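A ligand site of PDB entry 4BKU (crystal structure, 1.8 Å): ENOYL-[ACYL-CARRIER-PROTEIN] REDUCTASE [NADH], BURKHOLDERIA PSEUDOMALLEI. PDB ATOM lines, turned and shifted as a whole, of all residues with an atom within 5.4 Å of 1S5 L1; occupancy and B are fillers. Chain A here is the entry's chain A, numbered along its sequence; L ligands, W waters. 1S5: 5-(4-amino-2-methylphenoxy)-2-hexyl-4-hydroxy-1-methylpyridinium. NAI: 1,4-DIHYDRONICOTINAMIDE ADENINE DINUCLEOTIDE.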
ATOM      1  N   GLY A  93      -7.035  15.775  -2.192  1.00  0.00           N
ATOM      2  CA  GLY A  93      -8.234  15.196  -2.771  1.00  0.00           C
ATOM      3  C   GLY A  93      -7.892  13.870  -3.415  1.00  0.00           C
ATOM      4  O   GLY A  93      -6.783  13.700  -3.956  1.00  0.00           O
ATOM      5  N   PHE A  94      -8.818  12.911  -3.343  1.00  0.00           N
ATOM      6  CA  PHE A  94      -8.682  11.681  -4.097  1.00  0.00           C
ATOM      7  C   PHE A  94     -10.025  10.988  -4.259  1.00  0.00           C
ATOM      8  O   PHE A  94     -10.791  10.856  -3.296  1.00  0.00           O
ATOM      9  CB  PHE A  94      -7.719  10.681  -3.433  1.00  0.00           C
ATOM     10  CG  PHE A  94      -7.632   9.366  -4.161  1.00  0.00           C
ATOM     11  CD1 PHE A  94      -6.894   9.258  -5.335  1.00  0.00           C
ATOM     12  CD2 PHE A  94      -8.327   8.258  -3.702  1.00  0.00           C
ATOM     13  CE1 PHE A  94      -6.824   8.050  -6.025  1.00  0.00           C
ATOM     14  CE2 PHE A  94      -8.268   7.048  -4.383  1.00  0.00           C
ATOM     15  CZ  PHE A  94      -7.517   6.936  -5.553  1.00  0.00           C
ATOM     16  N   ALA A  95     -10.282  10.510  -5.472  1.00  0.00           N
ATOM     17  CA  ALA A  95     -11.364   9.555  -5.699  1.00  0.00           C
ATOM     18  C   ALA A  95     -10.876   8.516  -6.689  1.00  0.00           C
ATOM     19  O   ALA A  95     -10.130   8.847  -7.612  1.00  0.00           O
ATOM     20  CB  ALA A  95     -12.623  10.254  -6.197  1.00  0.00           C
ATOM     21  N   PRO A  96     -11.277   7.246  -6.505  1.00  0.00           N
ATOM     22  CA  PRO A  96     -10.834   6.186  -7.418  1.00  0.00           C
ATOM     23  C   PRO A  96     -11.226   6.496  -8.857  1.00  0.00           C
ATOM     24  O   PRO A  96     -12.295   7.070  -9.087  1.00  0.00           O
ATOM     25  CB  PRO A  96     -11.577   4.959  -6.895  1.00  0.00           C
ATOM     26  CG  PRO A  96     -11.732   5.241  -5.407  1.00  0.00           C
ATOM     27  CD  PRO A  96     -12.048   6.714  -5.371  1.00  0.00           C
ATOM     28  N   ILE A 100     -14.935   8.683 -10.874  1.00  0.00           N
ATOM     29  CA  ILE A 100     -14.971  10.020 -11.457  1.00  0.00           C
ATOM     30  C   ILE A 100     -14.837   9.981 -12.986  1.00  0.00           C
ATOM     31  O   ILE A 100     -14.272  10.881 -13.613  1.00  0.00           O
ATOM     32  CB  ILE A 100     -13.905  10.954 -10.863  1.00  0.00           C
ATOM     33  CG1 ILE A 100     -12.513  10.335 -10.987  1.00  0.00           C
ATOM     34  CG2 ILE A 100     -14.223  11.290  -9.393  1.00  0.00           C
ATOM     35  CD1 ILE A 100     -11.434  11.156 -10.295  1.00  0.00           C
ATOM     36  N   TYR A 146     -14.806  22.419  -5.244  1.00  0.00           N
ATOM     37  CA  TYR A 146     -15.086  22.640  -6.661  1.00  0.00           C
ATOM     38  C   TYR A 146     -16.579  22.738  -6.867  1.00  0.00           C
ATOM     39  O   TYR A 146     -17.342  22.189  -6.062  1.00  0.00           O
ATOM     40  CB  TYR A 146     -14.503  21.467  -7.487  1.00  0.00           C
ATOM     41  CG  TYR A 146     -14.794  21.556  -8.975  1.00  0.00           C
ATOM     42  CD1 TYR A 146     -14.380  22.662  -9.709  1.00  0.00           C
ATOM     43  CD2 TYR A 146     -15.490  20.540  -9.632  1.00  0.00           C
ATOM     44  CE1 TYR A 146     -14.654  22.751 -11.078  1.00  0.00           C
ATOM     45  CE2 TYR A 146     -15.762  20.622 -10.989  1.00  0.00           C
ATOM     46  CZ  TYR A 146     -15.337  21.725 -11.710  1.00  0.00           C
ATOM     47  OH  TYR A 146     -15.610  21.832 -13.061  1.00  0.00           O
ATOM     48  N   ILE A 153     -21.838  18.094 -12.283  1.00  0.00           N
ATOM     49  CA  ILE A 153     -20.923  18.307 -13.404  1.00  0.00           C
ATOM     50  C   ILE A 153     -20.501  16.936 -13.947  1.00  0.00           C
ATOM     51  O   ILE A 153     -20.187  16.031 -13.152  1.00  0.00           O
ATOM     52  CB  ILE A 153     -19.682  19.120 -12.954  1.00  0.00           C
ATOM     53  CG1 ILE A 153     -20.082  20.561 -12.671  1.00  0.00           C
ATOM     54  CG2 ILE A 153     -18.585  19.105 -14.020  1.00  0.00           C
ATOM     55  CD1 ILE A 153     -18.966  21.435 -12.126  1.00  0.00           C
ATOM     56  N   PRO A 154     -20.510  16.751 -15.273  1.00  0.00           N
ATOM     57  CA  PRO A 154     -20.203  15.436 -15.865  1.00  0.00           C
ATOM     58  C   PRO A 154     -18.881  14.874 -15.358  1.00  0.00           C
ATOM     59  O   PRO A 154     -17.894  15.613 -15.268  1.00  0.00           O
ATOM     60  CB  PRO A 154     -20.121  15.726 -17.366  1.00  0.00           C
ATOM     61  CG  PRO A 154     -21.048  16.902 -17.553  1.00  0.00           C
ATOM     62  CD  PRO A 154     -20.821  17.754 -16.316  1.00  0.00           C
ATOM     63  N   ASN A 155     -18.909  13.586 -14.999  1.00  0.00           N
ATOM     64  CA  ASN A 155     -17.753  12.859 -14.468  1.00  0.00           C
ATOM     65  C   ASN A 155     -17.371  13.125 -13.017  1.00  0.00           C
ATOM     66  O   ASN A 155     -16.688  12.288 -12.431  1.00  0.00           O
ATOM     67  CB  ASN A 155     -16.514  13.007 -15.375  1.00  0.00           C
ATOM     68  CG  ASN A 155     -16.782  12.607 -16.804  1.00  0.00           C
ATOM     69  OD1 ASN A 155     -17.340  11.528 -17.061  1.00  0.00           O
ATOM     70  ND2 ASN A 155     -16.393  13.448 -17.754  1.00  0.00           N
ATOM     71  N   TYR A 156     -17.755  14.263 -12.430  1.00  0.00           N
ATOM     72  CA  TYR A 156     -17.251  14.587 -11.098  1.00  0.00           C
ATOM     73  C   TYR A 156     -17.830  13.615 -10.084  1.00  0.00           C
ATOM     74  O   TYR A 156     -17.163  13.248  -9.111  1.00  0.00           O
ATOM     75  CB  TYR A 156     -17.563  16.047 -10.703  1.00  0.00           C
ATOM     76  CG  TYR A 156     -16.613  16.614  -9.657  1.00  0.00           C
ATOM     77  CD1 TYR A 156     -15.248  16.654  -9.885  1.00  0.00           C
ATOM     78  CD2 TYR A 156     -17.085  17.137  -8.459  1.00  0.00           C
ATOM     79  CE1 TYR A 156     -14.361  17.193  -8.943  1.00  0.00           C
ATOM     80  CE2 TYR A 156     -16.217  17.669  -7.510  1.00  0.00           C
ATOM     81  CZ  TYR A 156     -14.865  17.696  -7.759  1.00  0.00           C
ATOM     82  OH  TYR A 156     -14.007  18.245  -6.815  1.00  0.00           O
ATOM     83  N   MET A 159     -16.875  12.337  -6.397  1.00  0.00           N
ATOM     84  CA  MET A 159     -16.133  13.457  -5.812  1.00  0.00           C
ATOM     85  C   MET A 159     -17.059  14.648  -5.468  1.00  0.00           C
ATOM     86  O   MET A 159     -16.816  15.383  -4.487  1.00  0.00           O
ATOM     87  CB  MET A 159     -14.960  13.883  -6.725  1.00  0.00           C
ATOM     88  CG  MET A 159     -14.066  14.947  -6.114  1.00  0.00           C
ATOM     89  SD  MET A 159     -13.211  14.411  -4.604  1.00  0.00           S
ATOM     90  CE  MET A 159     -11.597  13.978  -5.256  1.00  0.00           C
ATOM     91  N   LYS A 163     -17.058  16.452  -1.886  1.00  0.00           N
ATOM     92  CA  LYS A 163     -16.880  17.895  -1.759  1.00  0.00           C
ATOM     93  C   LYS A 163     -18.071  18.575  -1.086  1.00  0.00           C
ATOM     94  O   LYS A 163     -17.894  19.577  -0.402  1.00  0.00           O
ATOM     95  CB  LYS A 163     -16.590  18.529  -3.111  1.00  0.00           C
ATOM     96  CG  LYS A 163     -15.235  18.167  -3.723  1.00  0.00           C
ATOM     97  CD  LYS A 163     -14.043  18.679  -2.902  1.00  0.00           C
ATOM     98  CE  LYS A 163     -12.721  18.384  -3.619  1.00  0.00           C
ATOM     99  NZ  LYS A 163     -11.519  18.842  -2.837  1.00  0.00           N
ATOM    100  N   PRO A 191     -11.268  25.165 -12.628  1.00  0.00           N
ATOM    101  CA  PRO A 191     -10.285  24.180 -13.103  1.00  0.00           C
ATOM    102  C   PRO A 191      -8.937  24.798 -13.448  1.00  0.00           C
ATOM    103  O   PRO A 191      -8.889  25.907 -14.008  1.00  0.00           O
ATOM    104  CB  PRO A 191     -10.938  23.605 -14.380  1.00  0.00           C
ATOM    105  CG  PRO A 191     -12.399  23.947 -14.259  1.00  0.00           C
ATOM    106  CD  PRO A 191     -12.458  25.242 -13.490  1.00  0.00           C
ATOM    107  N   ILE A 192      -7.859  24.080 -13.136  1.00  0.00           N
ATOM    108  CA  ILE A 192      -6.501  24.570 -13.390  1.00  0.00           C
ATOM    109  C   ILE A 192      -5.908  23.818 -14.589  1.00  0.00           C
ATOM    110  O   ILE A 192      -5.831  22.590 -14.572  1.00  0.00           O
ATOM    111  CB  ILE A 192      -5.599  24.341 -12.159  1.00  0.00           C
ATOM    112  CG1 ILE A 192      -6.151  25.091 -10.919  1.00  0.00           C
ATOM    113  CG2 ILE A 192      -4.131  24.703 -12.478  1.00  0.00           C
ATOM    114  CD1 ILE A 192      -6.338  26.593 -11.110  1.00  0.00           C
ATOM    115  N   GLY A 199      -5.849   8.501 -13.622  1.00  0.00           N
ATOM    116  CA  GLY A 199      -6.854   8.460 -12.586  1.00  0.00           C
ATOM    117  C   GLY A 199      -7.866   9.584 -12.700  1.00  0.00           C
ATOM    118  O   GLY A 199      -8.932   9.546 -12.077  1.00  0.00           O
ATOM    119  N   ILE A 200      -7.533  10.598 -13.488  1.00  0.00           N
ATOM    120  CA  ILE A 200      -8.438  11.719 -13.701  1.00  0.00           C
ATOM    121  C   ILE A 200      -8.760  11.825 -15.200  1.00  0.00           C
ATOM    122  O   ILE A 200      -7.861  11.760 -16.041  1.00  0.00           O
ATOM    123  CB  ILE A 200      -7.824  13.038 -13.205  1.00  0.00           C
ATOM    124  CG1 ILE A 200      -7.517  12.938 -11.701  1.00  0.00           C
ATOM    125  CG2 ILE A 200      -8.749  14.217 -13.498  1.00  0.00           C
ATOM    126  CD1 ILE A 200      -6.667  14.088 -11.190  1.00  0.00           C
ATOM    127  N   PHE A 203     -10.142  17.014 -18.713  1.00  0.00           N
ATOM    128  CA  PHE A 203     -11.134  18.062 -18.504  1.00  0.00           C
ATOM    129  C   PHE A 203     -10.902  19.226 -19.471  1.00  0.00           C
ATOM    130  O   PHE A 203     -11.267  20.362 -19.182  1.00  0.00           O
ATOM    131  CB  PHE A 203     -11.204  18.509 -17.028  1.00  0.00           C
ATOM    132  CG  PHE A 203      -9.873  18.851 -16.413  1.00  0.00           C
ATOM    133  CD1 PHE A 203      -9.023  17.855 -15.934  1.00  0.00           C
ATOM    134  CD2 PHE A 203      -9.478  20.188 -16.297  1.00  0.00           C
ATOM    135  CE1 PHE A 203      -7.781  18.184 -15.369  1.00  0.00           C
ATOM    136  CE2 PHE A 203      -8.251  20.523 -15.727  1.00  0.00           C
ATOM    137  CZ  PHE A 203      -7.400  19.507 -15.275  1.00  0.00           C
ATOM    138  N   ILE A 206     -14.033  21.080 -20.417  1.00  0.00           N
ATOM    139  CA  ILE A 206     -14.452  21.964 -19.329  1.00  0.00           C
ATOM    140  C   ILE A 206     -13.618  23.251 -19.319  1.00  0.00           C
ATOM    141  O   ILE A 206     -14.164  24.346 -19.138  1.00  0.00           O
ATOM    142  CB  ILE A 206     -14.384  21.230 -17.967  1.00  0.00           C
ATOM    143  CG1 ILE A 206     -15.468  20.148 -17.929  1.00  0.00           C
ATOM    144  CG2 ILE A 206     -14.560  22.219 -16.810  1.00  0.00           C
ATOM    145  CD1 ILE A 206     -15.466  19.345 -16.653  1.00  0.00           C
HETATM  146  OAA 1S5 L   1     -11.450  18.451  -7.410  1.00  0.00           O
HETATM  147  CAB 1S5 L   1     -10.924  18.619  -8.511  1.00  0.00           C
HETATM  148  CAC 1S5 L   1      -9.657  17.961  -8.825  1.00  0.00           C
HETATM  149  OAD 1S5 L   1      -8.938  17.328  -7.788  1.00  0.00           O
HETATM  150  CAE 1S5 L   1      -8.853  15.947  -7.907  1.00  0.00           C
HETATM  151  CAF 1S5 L   1      -7.784  15.292  -7.265  1.00  0.00           C
HETATM  152  CAG 1S5 L   1      -6.703  16.111  -6.582  1.00  0.00           C
HETATM  153  CAH 1S5 L   1     -11.582  19.363  -9.512  1.00  0.00           C
HETATM  154  CAI 1S5 L   1      -9.051  18.184 -10.063  1.00  0.00           C
HETATM  155  CAJ 1S5 L   1      -9.871  15.200  -8.495  1.00  0.00           C
HETATM  156  CAK 1S5 L   1      -7.701  13.886  -7.275  1.00  0.00           C
HETATM  157  CAL 1S5 L   1     -10.987  19.510 -10.791  1.00  0.00           C
HETATM  158  NAM 1S5 L   1      -9.712  18.953 -11.050  1.00  0.00           N
HETATM  159  CAN 1S5 L   1      -9.785  13.792  -8.514  1.00  0.00           C
HETATM  160  CAO 1S5 L   1      -8.690  13.139  -7.908  1.00  0.00           C
HETATM  161  NAP 1S5 L   1      -8.603  11.686  -7.928  1.00  0.00           N
HETATM  162  CAQ 1S5 L   1     -11.687  20.413 -11.844  1.00  0.00           C
HETATM  163  CAR 1S5 L   1      -9.084  19.130 -12.358  1.00  0.00           C
HETATM  164  CAS 1S5 L   1     -12.416  19.775 -12.980  1.00  0.00           C
HETATM  165  CAT 1S5 L   1     -13.009  18.408 -12.771  1.00  0.00           C
HETATM  166  CAU 1S5 L   1     -13.824  17.845 -13.901  1.00  0.00           C
HETATM  167  CAV 1S5 L   1     -15.075  17.110 -13.563  1.00  0.00           C
HETATM  168  CAW 1S5 L   1     -15.038  15.625 -13.683  1.00  0.00           C
HETATM  169  PA  NAI L   2      -2.672  17.777  -6.683  1.00  0.00           P
HETATM  170  O1A NAI L   2      -2.550  16.383  -7.198  1.00  0.00           O
HETATM  171  O2A NAI L   2      -1.380  18.437  -7.028  1.00  0.00           O
HETATM  172  O5B NAI L   2      -2.913  17.728  -5.120  1.00  0.00           O
HETATM  173  C5B NAI L   2      -3.631  16.634  -4.543  1.00  0.00           C
HETATM  174  C4B NAI L   2      -2.878  16.230  -3.303  1.00  0.00           C
HETATM  175  O4B NAI L   2      -3.630  15.327  -2.542  1.00  0.00           O
HETATM  176  C3B NAI L   2      -1.582  15.572  -3.663  1.00  0.00           C
HETATM  177  O3B NAI L   2      -0.531  16.179  -3.019  1.00  0.00           O
HETATM  178  C2B NAI L   2      -1.775  14.277  -3.069  1.00  0.00           C
HETATM  179  O2B NAI L   2      -0.483  13.741  -2.690  1.00  0.00           O
HETATM  180  C1B NAI L   2      -2.677  14.512  -1.938  1.00  0.00           C
HETATM  181  N9A NAI L   2      -3.234  13.263  -1.440  1.00  0.00           N
HETATM  182  C8A NAI L   2      -3.969  12.437  -2.133  1.00  0.00           C
HETATM  183  N7A NAI L   2      -4.250  11.319  -1.239  1.00  0.00           N
HETATM  184  C5A NAI L   2      -3.538  11.731  -0.021  1.00  0.00           C
HETATM  185  C6A NAI L   2      -3.403  10.997   1.273  1.00  0.00           C
HETATM  186  N6A NAI L   2      -3.982   9.692   1.474  1.00  0.00           N
HETATM  187  N1A NAI L   2      -2.689  11.532   2.248  1.00  0.00           N
HETATM  188  C2A NAI L   2      -2.075  12.872   2.070  1.00  0.00           C
HETATM  189  N3A NAI L   2      -2.215  13.515   0.751  1.00  0.00           N
HETATM  190  C4A NAI L   2      -2.984  12.886  -0.292  1.00  0.00           C
HETATM  191  O3  NAI L   2      -3.891  18.408  -7.388  1.00  0.00           O
HETATM  192  PN  NAI L   2      -4.541  19.817  -7.073  1.00  0.00           P
HETATM  193  O1N NAI L   2      -5.051  20.379  -8.371  1.00  0.00           O
HETATM  194  O2N NAI L   2      -3.531  20.820  -6.580  1.00  0.00           O
HETATM  195  O5D NAI L   2      -5.751  19.627  -6.047  1.00  0.00           O
HETATM  196  C5D NAI L   2      -5.668  20.224  -4.774  1.00  0.00           C
HETATM  197  C4D NAI L   2      -7.049  20.409  -4.206  1.00  0.00           C
HETATM  198  O4D NAI L   2      -7.785  21.293  -5.003  1.00  0.00           O
HETATM  199  C3D NAI L   2      -7.835  19.132  -4.186  1.00  0.00           C
HETATM  200  O3D NAI L   2      -8.658  19.095  -3.087  1.00  0.00           O
HETATM  201  C2D NAI L   2      -8.680  19.265  -5.374  1.00  0.00           C
HETATM  202  O2D NAI L   2      -9.827  18.453  -5.258  1.00  0.00           O
HETATM  203  C1D NAI L   2      -9.016  20.687  -5.323  1.00  0.00           C
HETATM  204  N1N NAI L   2      -9.408  21.295  -6.580  1.00  0.00           N
HETATM  205  C2N NAI L   2      -8.547  21.118  -7.722  1.00  0.00           C
HETATM  206  C3N NAI L   2      -8.977  21.848  -9.086  1.00  0.00           C
HETATM  207  C7N NAI L   2      -8.159  21.670 -10.238  1.00  0.00           C
HETATM  208  O7N NAI L   2      -8.797  22.119 -11.324  1.00  0.00           O
HETATM  209  N7N NAI L   2      -6.987  21.082  -9.950  1.00  0.00           N
HETATM  210  C4N NAI L   2     -10.231  22.638  -8.962  1.00  0.00           C
HETATM  211  C5N NAI L   2     -10.782  22.629  -7.793  1.00  0.00           C
HETATM  212  C6N NAI L   2     -10.391  22.044  -6.792  1.00  0.00           C
HETATM  213  O   HOH W   1     -11.812  15.179 -14.746  1.00  0.00           O
HETATM  214  O   HOH W   2      -8.144   8.858  -9.465  1.00  0.00           O
HETATM  215  O   HOH W   3      -5.871  17.764  -9.782  1.00  0.00           O
HETATM  216  O   HOH W   4      -5.742  10.359  -8.916  1.00  0.00           O
HETATM  217  O   HOH W   5     -13.442  15.758 -16.762  1.00  0.00           O
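A nitrogen (NAP) of 1S5 L1 is in hydrogen-bond range of the backbone carbonyl oxygen (O) of Ala 95, 3.2 Å away.
An oxygen (OAA) of 1S5 L1 is in hydrogen-bond range of the side-chain hydroxyl of Tyr 156, 2.6 Å away.
An oxygen (O3D) of NAI L2 lies within hydrogen-bond range of the side-chain amino group (NZ) of Lys 163, 2.9 Å away.
O7N of NAI L2 is in hydrogen-bond range of N of Ile 192 (2.8 Å).
The backbone NH (N) of Gly 93 lies within hydrogen-bond range of an oxygen (O4B) of NAI L2.
Merely in contact with 1S5 L1: Gly 93 (3.4 Å), Phe 94 (3.8 Å), Ile 100 (3.6 Å), Tyr 146 (3.7 Å), Pro 154 (3.3 Å), Asn 155 (3.4 Å), Met 159 (3.7 Å), Lys 163 (3.999 Å), Ile 200 (3.97 Å), Phe 203 (3.4 Å) and Ile 206 (3.5 Å).
O2D of NAI L2 is in hydrogen-bond range of OAA of 1S5 L1 (2.7 Å).
Water W2 lies within hydrogen-bond range of O of Ala 95 (2.7 Å), O of Gly 199 (2.8 Å) and NAP of 1S5 L1 (3.3 Å).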
